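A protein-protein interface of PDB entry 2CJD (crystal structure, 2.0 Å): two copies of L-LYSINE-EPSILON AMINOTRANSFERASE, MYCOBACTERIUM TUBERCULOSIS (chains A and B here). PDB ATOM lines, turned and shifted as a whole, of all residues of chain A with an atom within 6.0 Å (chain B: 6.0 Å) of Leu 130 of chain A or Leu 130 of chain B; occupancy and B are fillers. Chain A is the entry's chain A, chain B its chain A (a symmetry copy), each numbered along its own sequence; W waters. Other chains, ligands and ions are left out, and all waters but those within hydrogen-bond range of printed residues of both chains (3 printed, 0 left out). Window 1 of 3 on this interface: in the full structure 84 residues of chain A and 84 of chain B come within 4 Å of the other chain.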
ATOM      1  N   VAL A 125      31.906  22.663 -13.397  1.00  0.00           N
ATOM      2  CA  VAL A 125      31.136  22.747 -12.177  1.00  0.00           C
ATOM      3  C   VAL A 125      29.893  21.819 -12.360  1.00  0.00           C
ATOM      4  O   VAL A 125      29.533  21.449 -13.505  1.00  0.00           O
ATOM      5  CB  VAL A 125      30.768  24.218 -11.897  1.00  0.00           C
ATOM      6  CG1 VAL A 125      29.725  24.728 -12.901  1.00  0.00           C
ATOM      7  CG2 VAL A 125      30.265  24.417 -10.448  1.00  0.00           C
ATOM      8  N   GLU A 126      29.283  21.391 -11.262  1.00  0.00           N
ATOM      9  CA  GLU A 126      27.996  20.694 -11.358  1.00  0.00           C
ATOM     10  C   GLU A 126      26.866  21.734 -11.455  1.00  0.00           C
ATOM     11  O   GLU A 126      26.756  22.597 -10.595  1.00  0.00           O
ATOM     12  CB  GLU A 126      27.744  19.836 -10.126  1.00  0.00           C
ATOM     13  CG  GLU A 126      28.699  18.659  -9.929  1.00  0.00           C
ATOM     14  CD  GLU A 126      28.302  17.815  -8.694  1.00  0.00           C
ATOM     15  OE1 GLU A 126      27.829  18.382  -7.669  1.00  0.00           O
ATOM     16  OE2 GLU A 126      28.457  16.589  -8.769  1.00  0.00           O
ATOM     17  N   GLY A 127      26.044  21.650 -12.500  1.00  0.00           N
ATOM     18  CA  GLY A 127      24.791  22.429 -12.549  1.00  0.00           C
ATOM     19  C   GLY A 127      24.845  23.572 -13.554  1.00  0.00           C
ATOM     20  O   GLY A 127      25.839  24.313 -13.597  1.00  0.00           O
ATOM     21  N   GLY A 128      23.769  23.704 -14.346  1.00  0.00           N
ATOM     22  CA  GLY A 128      23.657  24.726 -15.378  1.00  0.00           C
ATOM     23  C   GLY A 128      23.577  26.139 -14.825  1.00  0.00           C
ATOM     24  O   GLY A 128      24.199  27.056 -15.361  1.00  0.00           O
ATOM     25  N   ALA A 129      22.803  26.336 -13.762  1.00  0.00           N
ATOM     26  CA  ALA A 129      22.692  27.683 -13.161  1.00  0.00           C
ATOM     27  C   ALA A 129      24.079  28.137 -12.657  1.00  0.00           C
ATOM     28  O   ALA A 129      24.458  29.284 -12.814  1.00  0.00           O
ATOM     29  CB  ALA A 129      21.694  27.688 -12.028  1.00  0.00           C
ATOM     30  N   LEU A 130      24.833  27.226 -12.067  1.00  0.00           N
ATOM     31  CA  LEU A 130      26.157  27.573 -11.557  1.00  0.00           C
ATOM     32  C   LEU A 130      27.169  27.825 -12.678  1.00  0.00           C
ATOM     33  O   LEU A 130      28.063  28.643 -12.507  1.00  0.00           O
ATOM     34  CB  LEU A 130      26.665  26.518 -10.602  1.00  0.00           C
ATOM     35  CG  LEU A 130      26.726  26.999  -9.147  1.00  0.00           C
ATOM     36  CD1 LEU A 130      25.622  27.979  -8.807  1.00  0.00           C
ATOM     37  CD2 LEU A 130      26.685  25.824  -8.227  1.00  0.00           C
ATOM     38  N   ALA A 131      26.999  27.161 -13.821  1.00  0.00           N
ATOM     39  CA  ALA A 131      27.802  27.493 -15.028  1.00  0.00           C
ATOM     40  C   ALA A 131      27.572  28.956 -15.425  1.00  0.00           C
ATOM     41  O   ALA A 131      28.531  29.714 -15.629  1.00  0.00           O
ATOM     42  CB  ALA A 131      27.486  26.551 -16.199  1.00  0.00           C
ATOM     43  N   VAL A 132      26.304  29.361 -15.508  1.00  0.00           N
ATOM     44  CA  VAL A 132      25.977  30.748 -15.832  1.00  0.00           C
ATOM     45  C   VAL A 132      26.521  31.682 -14.771  1.00  0.00           C
ATOM     46  O   VAL A 132      27.098  32.720 -15.116  1.00  0.00           O
ATOM     47  CB  VAL A 132      24.437  31.015 -16.046  1.00  0.00           C
ATOM     48  CG1 VAL A 132      24.189  32.490 -16.362  1.00  0.00           C
ATOM     49  CG2 VAL A 132      23.894  30.113 -17.189  1.00  0.00           C
ATOM     50  N   GLU A 133      26.372  31.322 -13.490  1.00  0.00           N
ATOM     51  CA  GLU A 133      26.880  32.175 -12.429  1.00  0.00           C
ATOM     52  C   GLU A 133      28.390  32.408 -12.488  1.00  0.00           C
ATOM     53  O   GLU A 133      28.863  33.496 -12.141  1.00  0.00           O
ATOM     54  CB  GLU A 133      26.532  31.622 -11.043  1.00  0.00           C
ATOM     55  CG  GLU A 133      25.068  31.755 -10.698  1.00  0.00           C
ATOM     56  CD  GLU A 133      24.850  31.921  -9.218  1.00  0.00           C
ATOM     57  OE1 GLU A 133      25.773  31.601  -8.449  1.00  0.00           O
ATOM     58  OE2 GLU A 133      23.740  32.339  -8.822  1.00  0.00           O
ATOM     59  N   ASN A 134      29.148  31.383 -12.862  1.00  0.00           N
ATOM     60  CA  ASN A 134      30.584  31.555 -12.964  1.00  0.00           C
ATOM     61  C   ASN A 134      30.989  32.430 -14.143  1.00  0.00           C
ATOM     62  O   ASN A 134      31.997  33.147 -14.068  1.00  0.00           O
ATOM     63  CB  ASN A 134      31.314  30.212 -12.992  1.00  0.00           C
ATOM     64  CG  ASN A 134      31.486  29.653 -11.629  1.00  0.00           C
ATOM     65  OD1 ASN A 134      32.379  30.074 -10.886  1.00  0.00           O
ATOM     66  ND2 ASN A 134      30.592  28.737 -11.246  1.00  0.00           N
ATOM     67  N   ALA A 135      30.206  32.369 -15.215  1.00  0.00           N
ATOM     68  CA  ALA A 135      30.353  33.283 -16.333  1.00  0.00           C
ATOM     69  C   ALA A 135      30.115  34.716 -15.841  1.00  0.00           C
ATOM     70  O   ALA A 135      30.895  35.613 -16.164  1.00  0.00           O
ATOM     71  CB  ALA A 135      29.387  32.934 -17.472  1.00  0.00           C
ATOM     72  N   SER A 171      19.112  30.018  -9.350  1.00  0.00           N
ATOM     73  CA  SER A 171      20.093  30.257  -8.277  1.00  0.00           C
ATOM     74  C   SER A 171      20.174  31.756  -7.952  1.00  0.00           C
ATOM     75  O   SER A 171      19.555  32.578  -8.633  1.00  0.00           O
ATOM     76  CB  SER A 171      21.473  29.710  -8.685  1.00  0.00           C
ATOM     77  OG  SER A 171      22.011  30.492  -9.746  1.00  0.00           O
ATOM     78  N   GLY A 172      20.947  32.126  -6.934  1.00  0.00           N
ATOM     79  CA  GLY A 172      20.939  33.513  -6.427  1.00  0.00           C
ATOM     80  C   GLY A 172      21.099  34.592  -7.484  1.00  0.00           C
ATOM     81  O   GLY A 172      20.330  35.557  -7.498  1.00  0.00           O
ATOM     82  N   VAL A 307      32.144  26.735 -18.078  1.00  0.00           N
ATOM     83  CA  VAL A 307      32.295  27.904 -18.939  1.00  0.00           C
ATOM     84  C   VAL A 307      33.530  27.738 -19.844  1.00  0.00           C
ATOM     85  O   VAL A 307      34.517  27.044 -19.470  1.00  0.00           O
ATOM     86  CB  VAL A 307      32.359  29.265 -18.129  1.00  0.00           C
ATOM     87  CG1 VAL A 307      31.177  29.383 -17.142  1.00  0.00           C
ATOM     88  CG2 VAL A 307      33.637  29.423 -17.368  1.00  0.00           C
ATOM     89  N   VAL B 125      19.609  18.122  -5.073  1.00  0.00           N
ATOM     90  CA  VAL B 125      20.172  18.999  -6.074  1.00  0.00           C
ATOM     91  C   VAL B 125      21.690  18.647  -6.182  1.00  0.00           C
ATOM     92  O   VAL B 125      22.266  18.010  -5.267  1.00  0.00           O
ATOM     93  CB  VAL B 125      19.907  20.467  -5.686  1.00  0.00           C
ATOM     94  CG1 VAL B 125      20.752  20.879  -4.471  1.00  0.00           C
ATOM     95  CG2 VAL B 125      20.161  21.428  -6.871  1.00  0.00           C
ATOM     96  N   GLU B 126      22.318  18.991  -7.300  1.00  0.00           N
ATOM     97  CA  GLU B 126      23.779  18.882  -7.387  1.00  0.00           C
ATOM     98  C   GLU B 126      24.414  20.140  -6.768  1.00  0.00           C
ATOM     99  O   GLU B 126      24.100  21.248  -7.179  1.00  0.00           O
ATOM    100  CB  GLU B 126      24.236  18.787  -8.836  1.00  0.00           C
ATOM    101  CG  GLU B 126      23.806  17.528  -9.588  1.00  0.00           C
ATOM    102  CD  GLU B 126      24.389  17.502 -11.020  1.00  0.00           C
ATOM    103  OE1 GLU B 126      24.510  18.578 -11.672  1.00  0.00           O
ATOM    104  OE2 GLU B 126      24.735  16.404 -11.474  1.00  0.00           O
ATOM    105  N   GLY B 127      25.293  19.960  -5.783  1.00  0.00           N
ATOM    106  CA  GLY B 127      26.140  21.071  -5.303  1.00  0.00           C
ATOM    107  C   GLY B 127      25.731  21.571  -3.925  1.00  0.00           C
ATOM    108  O   GLY B 127      24.534  21.773  -3.667  1.00  0.00           O
ATOM    109  N   GLY B 128      26.735  21.774  -3.056  1.00  0.00           N
ATOM    110  CA  GLY B 128      26.529  22.230  -1.687  1.00  0.00           C
ATOM    111  C   GLY B 128      25.999  23.650  -1.596  1.00  0.00           C
ATOM    112  O   GLY B 128      25.117  23.937  -0.786  1.00  0.00           O
ATOM    113  N   ALA B 129      26.535  24.556  -2.408  1.00  0.00           N
ATOM    114  CA  ALA B 129      26.056  25.955  -2.385  1.00  0.00           C
ATOM    115  C   ALA B 129      24.563  25.993  -2.776  1.00  0.00           C
ATOM    116  O   ALA B 129      23.780  26.722  -2.193  1.00  0.00           O
ATOM    117  CB  ALA B 129      26.867  26.820  -3.319  1.00  0.00           C
ATOM    118  N   LEU B 130      24.178  25.194  -3.756  1.00  0.00           N
ATOM    119  CA  LEU B 130      22.783  25.171  -4.192  1.00  0.00           C
ATOM    120  C   LEU B 130      21.858  24.517  -3.162  1.00  0.00           C
ATOM    121  O   LEU B 130      20.703  24.909  -3.058  1.00  0.00           O
ATOM    122  CB  LEU B 130      22.646  24.501  -5.540  1.00  0.00           C
ATOM    123  CG  LEU B 130      22.273  25.475  -6.663  1.00  0.00           C
ATOM    124  CD1 LEU B 130      22.868  26.854  -6.467  1.00  0.00           C
ATOM    125  CD2 LEU B 130      22.688  24.907  -7.980  1.00  0.00           C
ATOM    126  N   ALA B 131      22.376  23.564  -2.388  1.00  0.00           N
ATOM    127  CA  ALA B 131      21.618  23.022  -1.228  1.00  0.00           C
ATOM    128  C   ALA B 131      21.290  24.149  -0.241  1.00  0.00           C
ATOM    129  O   ALA B 131      20.133  24.310   0.171  1.00  0.00           O
ATOM    130  CB  ALA B 131      22.381  21.887  -0.530  1.00  0.00           C
ATOM    131  N   VAL B 132      22.299  24.944   0.115  1.00  0.00           N
ATOM    132  CA  VAL B 132      22.084  26.078   1.012  1.00  0.00           C
ATOM    133  C   VAL B 132      21.125  27.070   0.389  1.00  0.00           C
ATOM    134  O   VAL B 132      20.221  27.554   1.080  1.00  0.00           O
ATOM    135  CB  VAL B 132      23.410  26.812   1.454  1.00  0.00           C
ATOM    136  CG1 VAL B 132      23.085  27.989   2.373  1.00  0.00           C
ATOM    137  CG2 VAL B 132      24.361  25.810   2.164  1.00  0.00           C
ATOM    138  N   GLU B 133      21.288  27.365  -0.907  1.00  0.00           N
ATOM    139  CA  GLU B 133      20.394  28.306  -1.559  1.00  0.00           C
ATOM    140  C   GLU B 133      18.926  27.881  -1.544  1.00  0.00           C
ATOM    141  O   GLU B 133      18.035  28.732  -1.450  1.00  0.00           O
ATOM    142  CB  GLU B 133      20.806  28.563  -3.013  1.00  0.00           C
ATOM    143  CG  GLU B 133      22.064  29.389  -3.139  1.00  0.00           C
ATOM    144  CD  GLU B 133      22.066  30.224  -4.392  1.00  0.00           C
ATOM    145  OE1 GLU B 133      21.279  29.918  -5.304  1.00  0.00           O
ATOM    146  OE2 GLU B 133      22.884  31.166  -4.478  1.00  0.00           O
ATOM    147  N   ASN B 134      18.667  26.587  -1.698  1.00  0.00           N
ATOM    148  CA  ASN B 134      17.294  26.122  -1.662  1.00  0.00           C
ATOM    149  C   ASN B 134      16.685  26.193  -0.268  1.00  0.00           C
ATOM    150  O   ASN B 134      15.475  26.419  -0.128  1.00  0.00           O
ATOM    151  CB  ASN B 134      17.155  24.722  -2.258  1.00  0.00           C
ATOM    152  CG  ASN B 134      17.094  24.760  -3.740  1.00  0.00           C
ATOM    153  OD1 ASN B 134      16.046  25.063  -4.318  1.00  0.00           O
ATOM    154  ND2 ASN B 134      18.238  24.517  -4.387  1.00  0.00           N
ATOM    155  N   ALA B 135      17.521  26.007   0.747  1.00  0.00           N
ATOM    156  CA  ALA B 135      17.129  26.236   2.126  1.00  0.00           C
ATOM    157  C   ALA B 135      16.741  27.711   2.296  1.00  0.00           C
ATOM    158  O   ALA B 135      15.704  28.008   2.890  1.00  0.00           O
ATOM    159  CB  ALA B 135      18.251  25.857   3.099  1.00  0.00           C
ATOM    160  N   SER B 171      28.078  30.856  -4.550  1.00  0.00           N
ATOM    161  CA  SER B 171      26.991  31.113  -5.510  1.00  0.00           C
ATOM    162  C   SER B 171      26.300  32.446  -5.190  1.00  0.00           C
ATOM    163  O   SER B 171      26.605  33.081  -4.177  1.00  0.00           O
ATOM    164  CB  SER B 171      25.978  29.953  -5.490  1.00  0.00           C
ATOM    165  OG  SER B 171      25.273  29.943  -4.253  1.00  0.00           O
ATOM    166  N   GLY B 172      25.356  32.868  -6.027  1.00  0.00           N
ATOM    167  CA  GLY B 172      24.773  34.221  -5.912  1.00  0.00           C
ATOM    168  C   GLY B 172      24.299  34.606  -4.521  1.00  0.00           C
ATOM    169  O   GLY B 172      24.625  35.695  -4.040  1.00  0.00           O
ATOM    170  N   VAL B 307      18.211  19.433   0.833  1.00  0.00           N
ATOM    171  CA  VAL B 307      17.692  19.977   2.084  1.00  0.00           C
ATOM    172  C   VAL B 307      16.707  18.981   2.725  1.00  0.00           C
ATOM    173  O   VAL B 307      16.043  18.180   2.010  1.00  0.00           O
ATOM    174  CB  VAL B 307      17.028  21.406   1.908  1.00  0.00           C
ATOM    175  CG1 VAL B 307      17.976  22.375   1.169  1.00  0.00           C
ATOM    176  CG2 VAL B 307      15.727  21.349   1.171  1.00  0.00           C
HETATM  177  O   HOH W   1      26.826  15.439 -10.363  1.00  0.00           O
HETATM  178  O   HOH W   2      26.087  16.815  -6.038  1.00  0.00           O
HETATM  179  O   HOH W   3      26.573  18.650 -13.642  1.00  0.00           O
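The backbone NH (N) of Gly 172 of chain B sits at hydrogen-bond distance from the side-chain carboxylate (OE1) of Glu 133 of chain A, 2.8 Å away. N of Gly 172 of chain A lies within hydrogen-bond range of OE1 of Glu 133 of chain B, at 2.8 Å.
The side-chain amide nitrogen (ND2) of Asn 134 of chain A lies within hydrogen-bond range of the backbone carbonyl oxygen (O) of Leu 130 of chain A (2.8 Å). The side-chain hydroxyl (OG) of Ser 171 of chain A is in hydrogen-bond range of the side-chain carboxylate (OE2) of Glu 133 of chain A, at 2.7 Å. N of Gly 172 of chain A sits at hydrogen-bond distance from OE2 of Glu 133 of chain A. The backbone carbonyl oxygen of Leu 130 of chain B is in hydrogen-bond range of the side-chain amide nitrogen of Asn 134 of chain B. The side-chain carboxylate of Glu 133 of chain B lies within hydrogen-bond range of the side-chain hydroxyl of Ser 171 of chain B. OE2 of Glu 133 of chain B is in hydrogen-bond range of N of Gly 172 of chain B (3.4 Å).
Glu 126 of chain B touches Glu 126 of chain A. Glu 126 of chain A touches Gly 127 of chain B (OE1 to N, 3.5 Å). Gly 127 of chain A touches Glu 126 of chain B (N to OE1, 3.5 Å). Leu 130 of chain A touches Leu 130 of chain B. Ser 171 of chain B touches Leu 130 of chain A. Ser 171 of chain B touches Glu 133 of chain A. CB of Ser 171 of chain A touches CD1 of Leu 130 of chain B (3.9 Å). Glu 133 of chain B touches Ser 171 of chain A. Gly 172 of chain A touches Gly 172 of chain B (CA to CA, 3.9 Å).
Leu 130 of chain A touches two residues of chain B. Leu 130 of chain B touches two residues of chain A. Of the printed residues of chain A, Gly 127 of chain B touches Glu 126. Of the printed residues of chain B, Gly 172 of chain A touches Glu 133 and Gly 172. Printed residues of chain A within 4 Å of Glu 133 of chain B: Ser 171 (3.2 Å) and Gly 172 (2.8 Å). The nearest residue of chain A that does not touch Leu 130 of chain B is Ala 129 of chain A (5.0 Å).
Of the 14 printed residues of chain A, 6 touch a printed residue of chain B. Hydrophobic or aromatic side chains of chain A within 4 Å of the printed part of chain B: Leu 130. Printed residues of chain B that touch a printed residue of chain A: Glu 126, Gly 127, Leu 130, Glu 133, Ser 171 and Gly 172. Among the printed residues, no Asp or Glu carboxylate lies within 4 Å of a Lys or Arg side-chain nitrogen of the other chain.
Glu 126 of chain A touches its own counterpart, Glu 126 of chain B. Glu 126 of chain A touches Gly 127 of chain B, and with the chains exchanged Gly 127 of chain A touches Glu 126 of chain B. Leu 130 of chain A touches Ser 171 of chain B, and with the chains exchanged Ser 171 of chain A touches Leu 130 of chain B. Gly 172 of chain B touches its own counterpart, Gly 172 of chain A. Positions printed for both chains: 125, 126, 127, 128, 129, 130, 131, 132, 133, 134, 135, 171, 172 and 307. Of the 11 pairs that touch across the chains among the printed residues, 11 have their exchanged pair printed and touching as well.
Water W1 lies within hydrogen-bond range of OE2 of Glu 126 of chain A (2.6 Å) and OE2 of Glu 126 of chain B (2.6 Å). Water W3 bridges OE1 of Glu 126 of chain B and N of Gly 127 of chain A. Water W2 lies within hydrogen-bond range of OE1 of Glu 126 of chain A (2.9 Å) and N of Gly 127 of chain B (3.3 Å).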
